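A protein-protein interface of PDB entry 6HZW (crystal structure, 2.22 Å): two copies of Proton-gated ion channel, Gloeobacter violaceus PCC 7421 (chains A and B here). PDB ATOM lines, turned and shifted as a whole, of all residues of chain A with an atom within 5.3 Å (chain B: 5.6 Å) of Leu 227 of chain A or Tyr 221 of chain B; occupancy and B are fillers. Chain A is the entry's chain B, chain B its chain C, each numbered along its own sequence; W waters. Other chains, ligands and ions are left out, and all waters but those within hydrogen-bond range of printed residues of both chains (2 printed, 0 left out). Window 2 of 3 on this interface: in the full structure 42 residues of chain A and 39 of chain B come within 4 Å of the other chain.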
ATOM      1  N   ILE A 211      12.640   7.712  16.452  1.00  0.00           N
ATOM      2  CA  ILE A 211      12.889   8.900  15.659  1.00  0.00           C
ATOM      3  C   ILE A 211      11.720   9.887  15.787  1.00  0.00           C
ATOM      4  O   ILE A 211      11.951  11.105  15.892  1.00  0.00           O
ATOM      5  CB  ILE A 211      13.183   8.575  14.209  1.00  0.00           C
ATOM      6  CG1 ILE A 211      14.640   8.113  14.126  1.00  0.00           C
ATOM      7  CG2 ILE A 211      12.910   9.776  13.253  1.00  0.00           C
ATOM      8  CD1 ILE A 211      14.995   7.444  12.790  1.00  0.00           C
ATOM      9  N   SER A 212      10.482   9.374  15.814  1.00  0.00           N
ATOM     10  CA  SER A 212       9.306  10.219  16.010  1.00  0.00           C
ATOM     11  C   SER A 212       9.363  10.948  17.365  1.00  0.00           C
ATOM     12  O   SER A 212       8.732  12.000  17.514  1.00  0.00           O
ATOM     13  CB  SER A 212       7.978   9.453  15.888  1.00  0.00           C
ATOM     14  OG  SER A 212       7.511   8.799  17.054  1.00  0.00           O
ATOM     15  N   THR A 214      11.899  12.302  18.828  1.00  0.00           N
ATOM     16  CA  THR A 214      12.775  13.448  18.796  1.00  0.00           C
ATOM     17  C   THR A 214      11.977  14.777  18.764  1.00  0.00           C
ATOM     18  O   THR A 214      12.524  15.820  19.112  1.00  0.00           O
ATOM     19  CB  THR A 214      13.805  13.443  17.623  1.00  0.00           C
ATOM     20  OG1 THR A 214      13.138  13.499  16.354  1.00  0.00           O
ATOM     21  CG2 THR A 214      14.745  12.261  17.697  1.00  0.00           C
ATOM     22  N   ALA A 215      10.705  14.722  18.376  1.00  0.00           N
ATOM     23  CA  ALA A 215       9.772  15.807  18.355  1.00  0.00           C
ATOM     24  C   ALA A 215       9.551  16.407  19.762  1.00  0.00           C
ATOM     25  O   ALA A 215       9.081  17.566  19.876  1.00  0.00           O
ATOM     26  CB  ALA A 215       8.427  15.353  17.754  1.00  0.00           C
ATOM     27  N   SER A 218      11.917  19.379  20.318  1.00  0.00           N
ATOM     28  CA  SER A 218      11.752  20.394  19.288  1.00  0.00           C
ATOM     29  C   SER A 218      10.493  21.220  19.499  1.00  0.00           C
ATOM     30  O   SER A 218       9.433  20.683  19.812  1.00  0.00           O
ATOM     31  CB  SER A 218      11.705  19.731  17.896  1.00  0.00           C
ATOM     32  OG  SER A 218      11.078  20.557  16.908  1.00  0.00           O
ATOM     33  N   SER A 220       9.784  23.397  16.884  1.00  0.00           N
ATOM     34  CA  SER A 220       9.341  23.621  15.516  1.00  0.00           C
ATOM     35  C   SER A 220       8.165  22.670  15.169  1.00  0.00           C
ATOM     36  O   SER A 220       8.376  21.476  14.942  1.00  0.00           O
ATOM     37  CB  SER A 220      10.514  23.449  14.571  1.00  0.00           C
ATOM     38  OG  SER A 220      10.064  23.359  13.233  1.00  0.00           O
ATOM     39  N   ALA A 223       8.467  20.956  11.629  1.00  0.00           N
ATOM     40  CA  ALA A 223       9.432  19.877  11.664  1.00  0.00           C
ATOM     41  C   ALA A 223       8.860  18.652  12.414  1.00  0.00           C
ATOM     42  O   ALA A 223       9.099  17.514  12.022  1.00  0.00           O
ATOM     43  CB  ALA A 223      10.704  20.302  12.348  1.00  0.00           C
ATOM     44  N   ASN A 224       8.128  18.924  13.488  1.00  0.00           N
ATOM     45  CA  ASN A 224       7.461  17.914  14.320  1.00  0.00           C
ATOM     46  C   ASN A 224       6.412  17.144  13.497  1.00  0.00           C
ATOM     47  O   ASN A 224       6.372  15.926  13.594  1.00  0.00           O
ATOM     48  CB  ASN A 224       6.828  18.559  15.556  1.00  0.00           C
ATOM     49  CG  ASN A 224       7.869  19.029  16.555  1.00  0.00           C
ATOM     50  OD1 ASN A 224       9.050  18.783  16.382  1.00  0.00           O
ATOM     51  ND2 ASN A 224       7.429  19.679  17.612  1.00  0.00           N
ATOM     52  N   VAL A 225       5.572  17.853  12.750  1.00  0.00           N
ATOM     53  CA  VAL A 225       4.555  17.271  11.911  1.00  0.00           C
ATOM     54  C   VAL A 225       5.249  16.345  10.860  1.00  0.00           C
ATOM     55  O   VAL A 225       4.823  15.208  10.681  1.00  0.00           O
ATOM     56  CB  VAL A 225       3.649  18.359  11.290  1.00  0.00           C
ATOM     57  CG1 VAL A 225       2.943  17.861  10.062  1.00  0.00           C
ATOM     58  CG2 VAL A 225       2.635  18.844  12.308  1.00  0.00           C
ATOM     59  N   THR A 226       6.359  16.802  10.273  1.00  0.00           N
ATOM     60  CA  THR A 226       7.150  16.045   9.338  1.00  0.00           C
ATOM     61  C   THR A 226       7.734  14.782   9.987  1.00  0.00           C
ATOM     62  O   THR A 226       7.667  13.701   9.381  1.00  0.00           O
ATOM     63  CB  THR A 226       8.249  16.929   8.703  1.00  0.00           C
ATOM     64  OG1 THR A 226       7.582  17.931   7.915  1.00  0.00           O
ATOM     65  CG2 THR A 226       9.192  16.086   7.808  1.00  0.00           C
ATOM     66  N   LEU A 227       8.263  14.904  11.203  1.00  0.00           N
ATOM     67  CA  LEU A 227       8.825  13.777  11.943  1.00  0.00           C
ATOM     68  C   LEU A 227       7.796  12.685  12.257  1.00  0.00           C
ATOM     69  O   LEU A 227       8.074  11.529  12.032  1.00  0.00           O
ATOM     70  CB  LEU A 227       9.441  14.204  13.265  1.00  0.00           C
ATOM     71  CG  LEU A 227      10.912  14.648  13.225  1.00  0.00           C
ATOM     72  CD1 LEU A 227      11.197  15.549  14.441  1.00  0.00           C
ATOM     73  CD2 LEU A 227      11.877  13.481  13.205  1.00  0.00           C
ATOM     74  N   VAL A 228       6.647  13.054  12.832  1.00  0.00           N
ATOM     75  CA  VAL A 228       5.632  12.118  13.281  1.00  0.00           C
ATOM     76  C   VAL A 228       4.826  11.486  12.103  1.00  0.00           C
ATOM     77  O   VAL A 228       4.619  10.273  12.111  1.00  0.00           O
ATOM     78  CB  VAL A 228       4.758  12.766  14.364  1.00  0.00           C
ATOM     79  CG1 VAL A 228       3.819  11.732  14.961  1.00  0.00           C
ATOM     80  CG2 VAL A 228       5.670  13.303  15.504  1.00  0.00           C
ATOM     81  N   VAL A 229       4.447  12.292  11.109  1.00  0.00           N
ATOM     82  CA  VAL A 229       3.697  11.828   9.975  1.00  0.00           C
ATOM     83  C   VAL A 229       4.520  10.909   9.034  1.00  0.00           C
ATOM     84  O   VAL A 229       4.022   9.855   8.617  1.00  0.00           O
ATOM     85  CB  VAL A 229       3.006  12.994   9.281  1.00  0.00           C
ATOM     86  CG1 VAL A 229       2.266  12.539   8.042  1.00  0.00           C
ATOM     87  CG2 VAL A 229       1.977  13.572  10.290  1.00  0.00           C
ATOM     88  N   SER A 230       5.762  11.269   8.754  1.00  0.00           N
ATOM     89  CA  SER A 230       6.649  10.480   7.901  1.00  0.00           C
ATOM     90  C   SER A 230       6.960   9.101   8.487  1.00  0.00           C
ATOM     91  O   SER A 230       6.950   8.106   7.745  1.00  0.00           O
ATOM     92  CB  SER A 230       7.980  11.228   7.674  1.00  0.00           C
ATOM     93  OG  SER A 230       7.677  12.439   6.979  1.00  0.00           O
ATOM     94  N   THR A 231       7.259   9.052   9.800  1.00  0.00           N
ATOM     95  CA  THR A 231       7.547   7.821  10.500  1.00  0.00           C
ATOM     96  C   THR A 231       6.292   6.927  10.596  1.00  0.00           C
ATOM     97  O   THR A 231       6.433   5.690  10.523  1.00  0.00           O
ATOM     98  CB  THR A 231       8.157   8.048  11.896  1.00  0.00           C
ATOM     99  OG1 THR A 231       7.363   8.971  12.662  1.00  0.00           O
ATOM    100  CG2 THR A 231       9.572   8.531  11.735  1.00  0.00           C
ATOM    101  N   LEU A 232       5.096   7.552  10.731  1.00  0.00           N
ATOM    102  CA  LEU A 232       3.835   6.843  10.782  1.00  0.00           C
ATOM    103  C   LEU A 232       3.608   6.098   9.432  1.00  0.00           C
ATOM    104  O   LEU A 232       3.172   4.951   9.434  1.00  0.00           O
ATOM    105  CB  LEU A 232       2.680   7.789  11.073  1.00  0.00           C
ATOM    106  CG  LEU A 232       1.259   7.219  10.895  1.00  0.00           C
ATOM    107  CD1 LEU A 232       1.001   6.020  11.738  1.00  0.00           C
ATOM    108  CD2 LEU A 232       0.244   8.231  11.286  1.00  0.00           C
ATOM    109  N   SER B 218      24.161  22.274   6.883  1.00  0.00           N
ATOM    110  CA  SER B 218      22.948  23.047   6.996  1.00  0.00           C
ATOM    111  C   SER B 218      22.536  23.286   8.445  1.00  0.00           C
ATOM    112  O   SER B 218      22.604  22.372   9.269  1.00  0.00           O
ATOM    113  CB  SER B 218      21.794  22.314   6.254  1.00  0.00           C
ATOM    114  OG  SER B 218      20.479  22.745   6.714  1.00  0.00           O
ATOM    115  N   THR B 219      22.104  24.535   8.701  1.00  0.00           N
ATOM    116  CA  THR B 219      21.599  25.003  10.004  1.00  0.00           C
ATOM    117  C   THR B 219      20.062  24.994  10.009  1.00  0.00           C
ATOM    118  O   THR B 219      19.459  25.227  11.046  1.00  0.00           O
ATOM    119  CB  THR B 219      22.165  26.448  10.360  1.00  0.00           C
ATOM    120  OG1 THR B 219      22.217  27.272   9.178  1.00  0.00           O
ATOM    121  CG2 THR B 219      23.608  26.323  10.838  1.00  0.00           C
ATOM    122  N   SER B 220      19.415  24.754   8.862  1.00  0.00           N
ATOM    123  CA  SER B 220      17.969  24.686   8.775  1.00  0.00           C
ATOM    124  C   SER B 220      17.467  23.309   9.278  1.00  0.00           C
ATOM    125  O   SER B 220      17.594  22.302   8.577  1.00  0.00           O
ATOM    126  CB  SER B 220      17.506  24.971   7.371  1.00  0.00           C
ATOM    127  OG  SER B 220      16.138  24.600   7.204  1.00  0.00           O
ATOM    128  N   TYR B 221      16.914  23.291  10.490  1.00  0.00           N
ATOM    129  CA  TYR B 221      16.324  22.109  11.123  1.00  0.00           C
ATOM    130  C   TYR B 221      15.215  21.429  10.284  1.00  0.00           C
ATOM    131  O   TYR B 221      15.218  20.217  10.119  1.00  0.00           O
ATOM    132  CB  TYR B 221      15.727  22.462  12.483  1.00  0.00           C
ATOM    133  CG  TYR B 221      15.169  21.277  13.268  1.00  0.00           C
ATOM    134  CD1 TYR B 221      15.898  20.129  13.455  1.00  0.00           C
ATOM    135  CD2 TYR B 221      13.917  21.329  13.859  1.00  0.00           C
ATOM    136  CE1 TYR B 221      15.400  19.055  14.196  1.00  0.00           C
ATOM    137  CE2 TYR B 221      13.428  20.274  14.592  1.00  0.00           C
ATOM    138  CZ  TYR B 221      14.165  19.132  14.746  1.00  0.00           C
ATOM    139  OH  TYR B 221      13.627  18.076  15.485  1.00  0.00           O
ATOM    140  N   GLU B 222      14.312  22.244   9.750  1.00  0.00           N
ATOM    141  CA  GLU B 222      13.151  21.849   8.974  1.00  0.00           C
ATOM    142  C   GLU B 222      13.636  21.100   7.690  1.00  0.00           C
ATOM    143  O   GLU B 222      13.034  20.061   7.301  1.00  0.00           O
ATOM    144  CB  GLU B 222      12.244  23.072   8.666  1.00  0.00           C
ATOM    145  CG  GLU B 222      11.676  23.916   9.886  1.00  0.00           C
ATOM    146  CD  GLU B 222      12.690  24.783  10.821  1.00  0.00           C
ATOM    147  OE1 GLU B 222      13.779  25.278  10.360  1.00  0.00           O
ATOM    148  OE2 GLU B 222      12.390  24.999  12.073  1.00  0.00           O
ATOM    149  N   ALA B 223      14.686  21.637   7.045  1.00  0.00           N
ATOM    150  CA  ALA B 223      15.263  21.079   5.839  1.00  0.00           C
ATOM    151  C   ALA B 223      16.039  19.778   6.162  1.00  0.00           C
ATOM    152  O   ALA B 223      16.010  18.818   5.379  1.00  0.00           O
ATOM    153  CB  ALA B 223      16.204  22.055   5.185  1.00  0.00           C
ATOM    154  N   ASN B 224      16.743  19.790   7.298  1.00  0.00           N
ATOM    155  CA  ASN B 224      17.513  18.656   7.795  1.00  0.00           C
ATOM    156  C   ASN B 224      16.598  17.466   8.088  1.00  0.00           C
ATOM    157  O   ASN B 224      16.945  16.349   7.720  1.00  0.00           O
ATOM    158  CB  ASN B 224      18.309  19.063   9.054  1.00  0.00           C
ATOM    159  CG  ASN B 224      19.462  19.987   8.735  1.00  0.00           C
ATOM    160  OD1 ASN B 224      19.736  20.248   7.576  1.00  0.00           O
ATOM    161  ND2 ASN B 224      20.144  20.470   9.762  1.00  0.00           N
ATOM    162  N   VAL B 225      15.487  17.694   8.780  1.00  0.00           N
ATOM    163  CA  VAL B 225      14.511  16.675   9.115  1.00  0.00           C
ATOM    164  C   VAL B 225      13.980  16.058   7.799  1.00  0.00           C
ATOM    165  O   VAL B 225      13.926  14.835   7.673  1.00  0.00           O
ATOM    166  CB  VAL B 225      13.427  17.224  10.056  1.00  0.00           C
ATOM    167  CG1 VAL B 225      12.219  16.339  10.043  1.00  0.00           C
ATOM    168  CG2 VAL B 225      13.964  17.293  11.489  1.00  0.00           C
ATOM    169  N   THR B 226      13.684  16.899   6.796  1.00  0.00           N
ATOM    170  CA  THR B 226      13.237  16.477   5.490  1.00  0.00           C
ATOM    171  C   THR B 226      14.298  15.627   4.782  1.00  0.00           C
ATOM    172  O   THR B 226      13.957  14.581   4.217  1.00  0.00           O
ATOM    173  CB  THR B 226      12.799  17.683   4.658  1.00  0.00           C
ATOM    174  OG1 THR B 226      11.631  18.256   5.299  1.00  0.00           O
ATOM    175  CG2 THR B 226      12.452  17.250   3.186  1.00  0.00           C
ATOM    176  N   VAL B 229      14.835  12.075   7.088  1.00  0.00           N
ATOM    177  CA  VAL B 229      13.656  11.259   7.107  1.00  0.00           C
ATOM    178  C   VAL B 229      13.256  10.714   5.720  1.00  0.00           C
ATOM    179  O   VAL B 229      12.947   9.526   5.606  1.00  0.00           O
ATOM    180  CB  VAL B 229      12.531  11.962   7.877  1.00  0.00           C
ATOM    181  CG1 VAL B 229      11.259  11.173   7.855  1.00  0.00           C
ATOM    182  CG2 VAL B 229      12.991  12.117   9.332  1.00  0.00           C
ATOM    183  N   VAL B 270      19.827  11.669  12.873  1.00  0.00           N
ATOM    184  CA  VAL B 270      18.639  12.315  13.425  1.00  0.00           C
ATOM    185  C   VAL B 270      18.986  12.936  14.829  1.00  0.00           C
ATOM    186  O   VAL B 270      18.614  14.085  15.089  1.00  0.00           O
ATOM    187  CB  VAL B 270      17.417  11.360  13.502  1.00  0.00           C
ATOM    188  CG1 VAL B 270      16.273  12.006  14.271  1.00  0.00           C
ATOM    189  CG2 VAL B 270      16.947  10.994  12.080  1.00  0.00           C
ATOM    190  N   VAL B 273      21.075  16.084  14.210  1.00  0.00           N
ATOM    191  CA  VAL B 273      20.190  17.123  13.692  1.00  0.00           C
ATOM    192  C   VAL B 273      19.311  17.720  14.831  1.00  0.00           C
ATOM    193  O   VAL B 273      19.105  18.960  14.867  1.00  0.00           O
ATOM    194  CB  VAL B 273      19.414  16.590  12.474  1.00  0.00           C
ATOM    195  CG1 VAL B 273      18.181  17.413  12.235  1.00  0.00           C
ATOM    196  CG2 VAL B 273      20.328  16.605  11.253  1.00  0.00           C
ATOM    197  N   THR B 274      18.862  16.866  15.762  1.00  0.00           N
ATOM    198  CA  THR B 274      18.052  17.245  16.908  1.00  0.00           C
ATOM    199  C   THR B 274      18.911  18.075  17.907  1.00  0.00           C
ATOM    200  O   THR B 274      18.465  19.137  18.343  1.00  0.00           O
ATOM    201  CB  THR B 274      17.530  16.000  17.606  1.00  0.00           C
ATOM    202  OG1 THR B 274      16.795  15.150  16.671  1.00  0.00           O
ATOM    203  CG2 THR B 274      16.665  16.372  18.762  1.00  0.00           C
ATOM    204  N   HIS B 277      19.774  21.618  16.504  1.00  0.00           N
ATOM    205  CA  HIS B 277      18.632  22.511  16.648  1.00  0.00           C
ATOM    206  C   HIS B 277      18.403  22.954  18.132  1.00  0.00           C
ATOM    207  O   HIS B 277      18.183  24.114  18.389  1.00  0.00           O
ATOM    208  CB  HIS B 277      17.383  21.854  16.131  1.00  0.00           C
ATOM    209  CG  HIS B 277      16.143  22.674  16.278  1.00  0.00           C
ATOM    210  ND1 HIS B 277      15.921  23.835  15.549  1.00  0.00           N
ATOM    211  CD2 HIS B 277      15.064  22.506  17.063  1.00  0.00           C
ATOM    212  CE1 HIS B 277      14.748  24.335  15.876  1.00  0.00           C
ATOM    213  NE2 HIS B 277      14.204  23.543  16.789  1.00  0.00           N
HETATM  214  O   HOH W   1      14.603  15.585  15.185  1.00  0.00           O
HETATM  215  O   HOH W   2      10.285  19.643   7.759  1.00  0.00           O
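The side-chain hydroxyl of Ser 220 of chain A lies within hydrogen-bond range of the side-chain carboxylate of Glu 222 of chain B (3.1 Å).
OG of Ser 220 of chain A sits close to N of Ala 223 of chain A (3.3 Å). O of Leu 227 of chain A lies within hydrogen-bond range of OG1 of Thr 231 of chain A. OD1 of Asn 224 of chain A sits at hydrogen-bond distance from OG of Ser 218 of chain A (2.7 Å). O of Thr 226 of chain A sits at hydrogen-bond distance from OG of Ser 230 of chain A. The backbone carbonyl oxygen (O) of Ser 220 of chain A sits close to the side-chain amide oxygen (OD1) of Asn 224 of chain A, 3.1 Å away. O of Glu 222 of chain B sits at hydrogen-bond distance from OG1 of Thr 226 of chain B (3.0 Å).
Among the printed residues, merely in contact across the chains: Ser 230 of chain A with Val 229 of chain B (3.3 Å), Ser 218 of chain A with Tyr 221 of chain B (3.3 Å), Ala 223 of chain A with Tyr 221 of chain B (3.5 Å), Thr 214 of chain A with Thr 274 of chain B (3.6 Å), Leu 227 of chain A with Tyr 221 of chain B (3.7 Å), Thr 214 of chain A with Val 270 of chain B (3.8 Å), Thr 226 of chain A with Val 225 of chain B (3.8 Å), Leu 227 of chain A with Val 225 of chain B (3.8 Å) and Ala 223 of chain A with Val 225 of chain B (3.9 Å).
Ile 211 of chain A touches none of the printed residues of chain B. Printed residues of chain B within 4 Å of Thr 214 of chain A: Val 270 and Thr 274. Of the printed residues of chain B, Ser 220 of chain A touches Glu 222 (3.1 Å). Asn 224 of chain A touches none of the printed residues of chain B. Printed residues of chain B within 4 Å of Thr 226 of chain A: Val 225 (3.8 Å). Of chain B, only Tyr 221 and Val 225 come within 4 Å of Leu 227 of chain A. Of chain A, only Ser 218, Ala 223 and Leu 227 come within 4 Å of Tyr 221 of chain B. Of the printed residues of chain A, Thr 274 of chain B touches Thr 214. The nearest residue of chain B that does not touch Leu 227 of chain A is Val 229 of chain B (4.3 Å). The nearest residue of chain A that does not touch Tyr 221 of chain B is Ser 220 of chain A (4.1 Å).
Hydrophobic or aromatic side chains of chain B that line the printed part of chain A: Tyr 221, Val 225, Val 229 and Val 270. Hydrophobic or aromatic side chains of chain A within 4 Å of the printed part of chain B: Ala 223 and Leu 227. Among the printed residues, no Asp or Glu carboxylate lies within 4 Å of a Lys or Arg side-chain nitrogen of the other chain.
Ala 223 of chain A touches Val 225 of chain B, but with the chains exchanged Val 225 of chain A does not touch Ala 223 of chain B (11.4 Å). Thr 226 of chain A touches Val 225 of chain B, but with the chains exchanged Val 225 of chain A does not touch Thr 226 of chain B (8.7 Å). Of the 10 pairs that touch across the chains among the printed residues, none has its exchanged pair printed and touching as well.
Water W1 lies within hydrogen-bond range of OG1 of Thr 274 of chain B (2.7 Å), OH of Tyr 221 of chain B (2.7 Å) and OG1 of Thr 214 of chain A (2.8 Å). Water W2 lies within hydrogen-bond range of the backbone carbonyl oxygen of Glu 222 of chain B (2.8 Å), the side-chain hydroxyl of Thr 226 of chain B (3.1 Å) and the side-chain hydroxyl of Thr 226 of chain A (3.2 Å).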
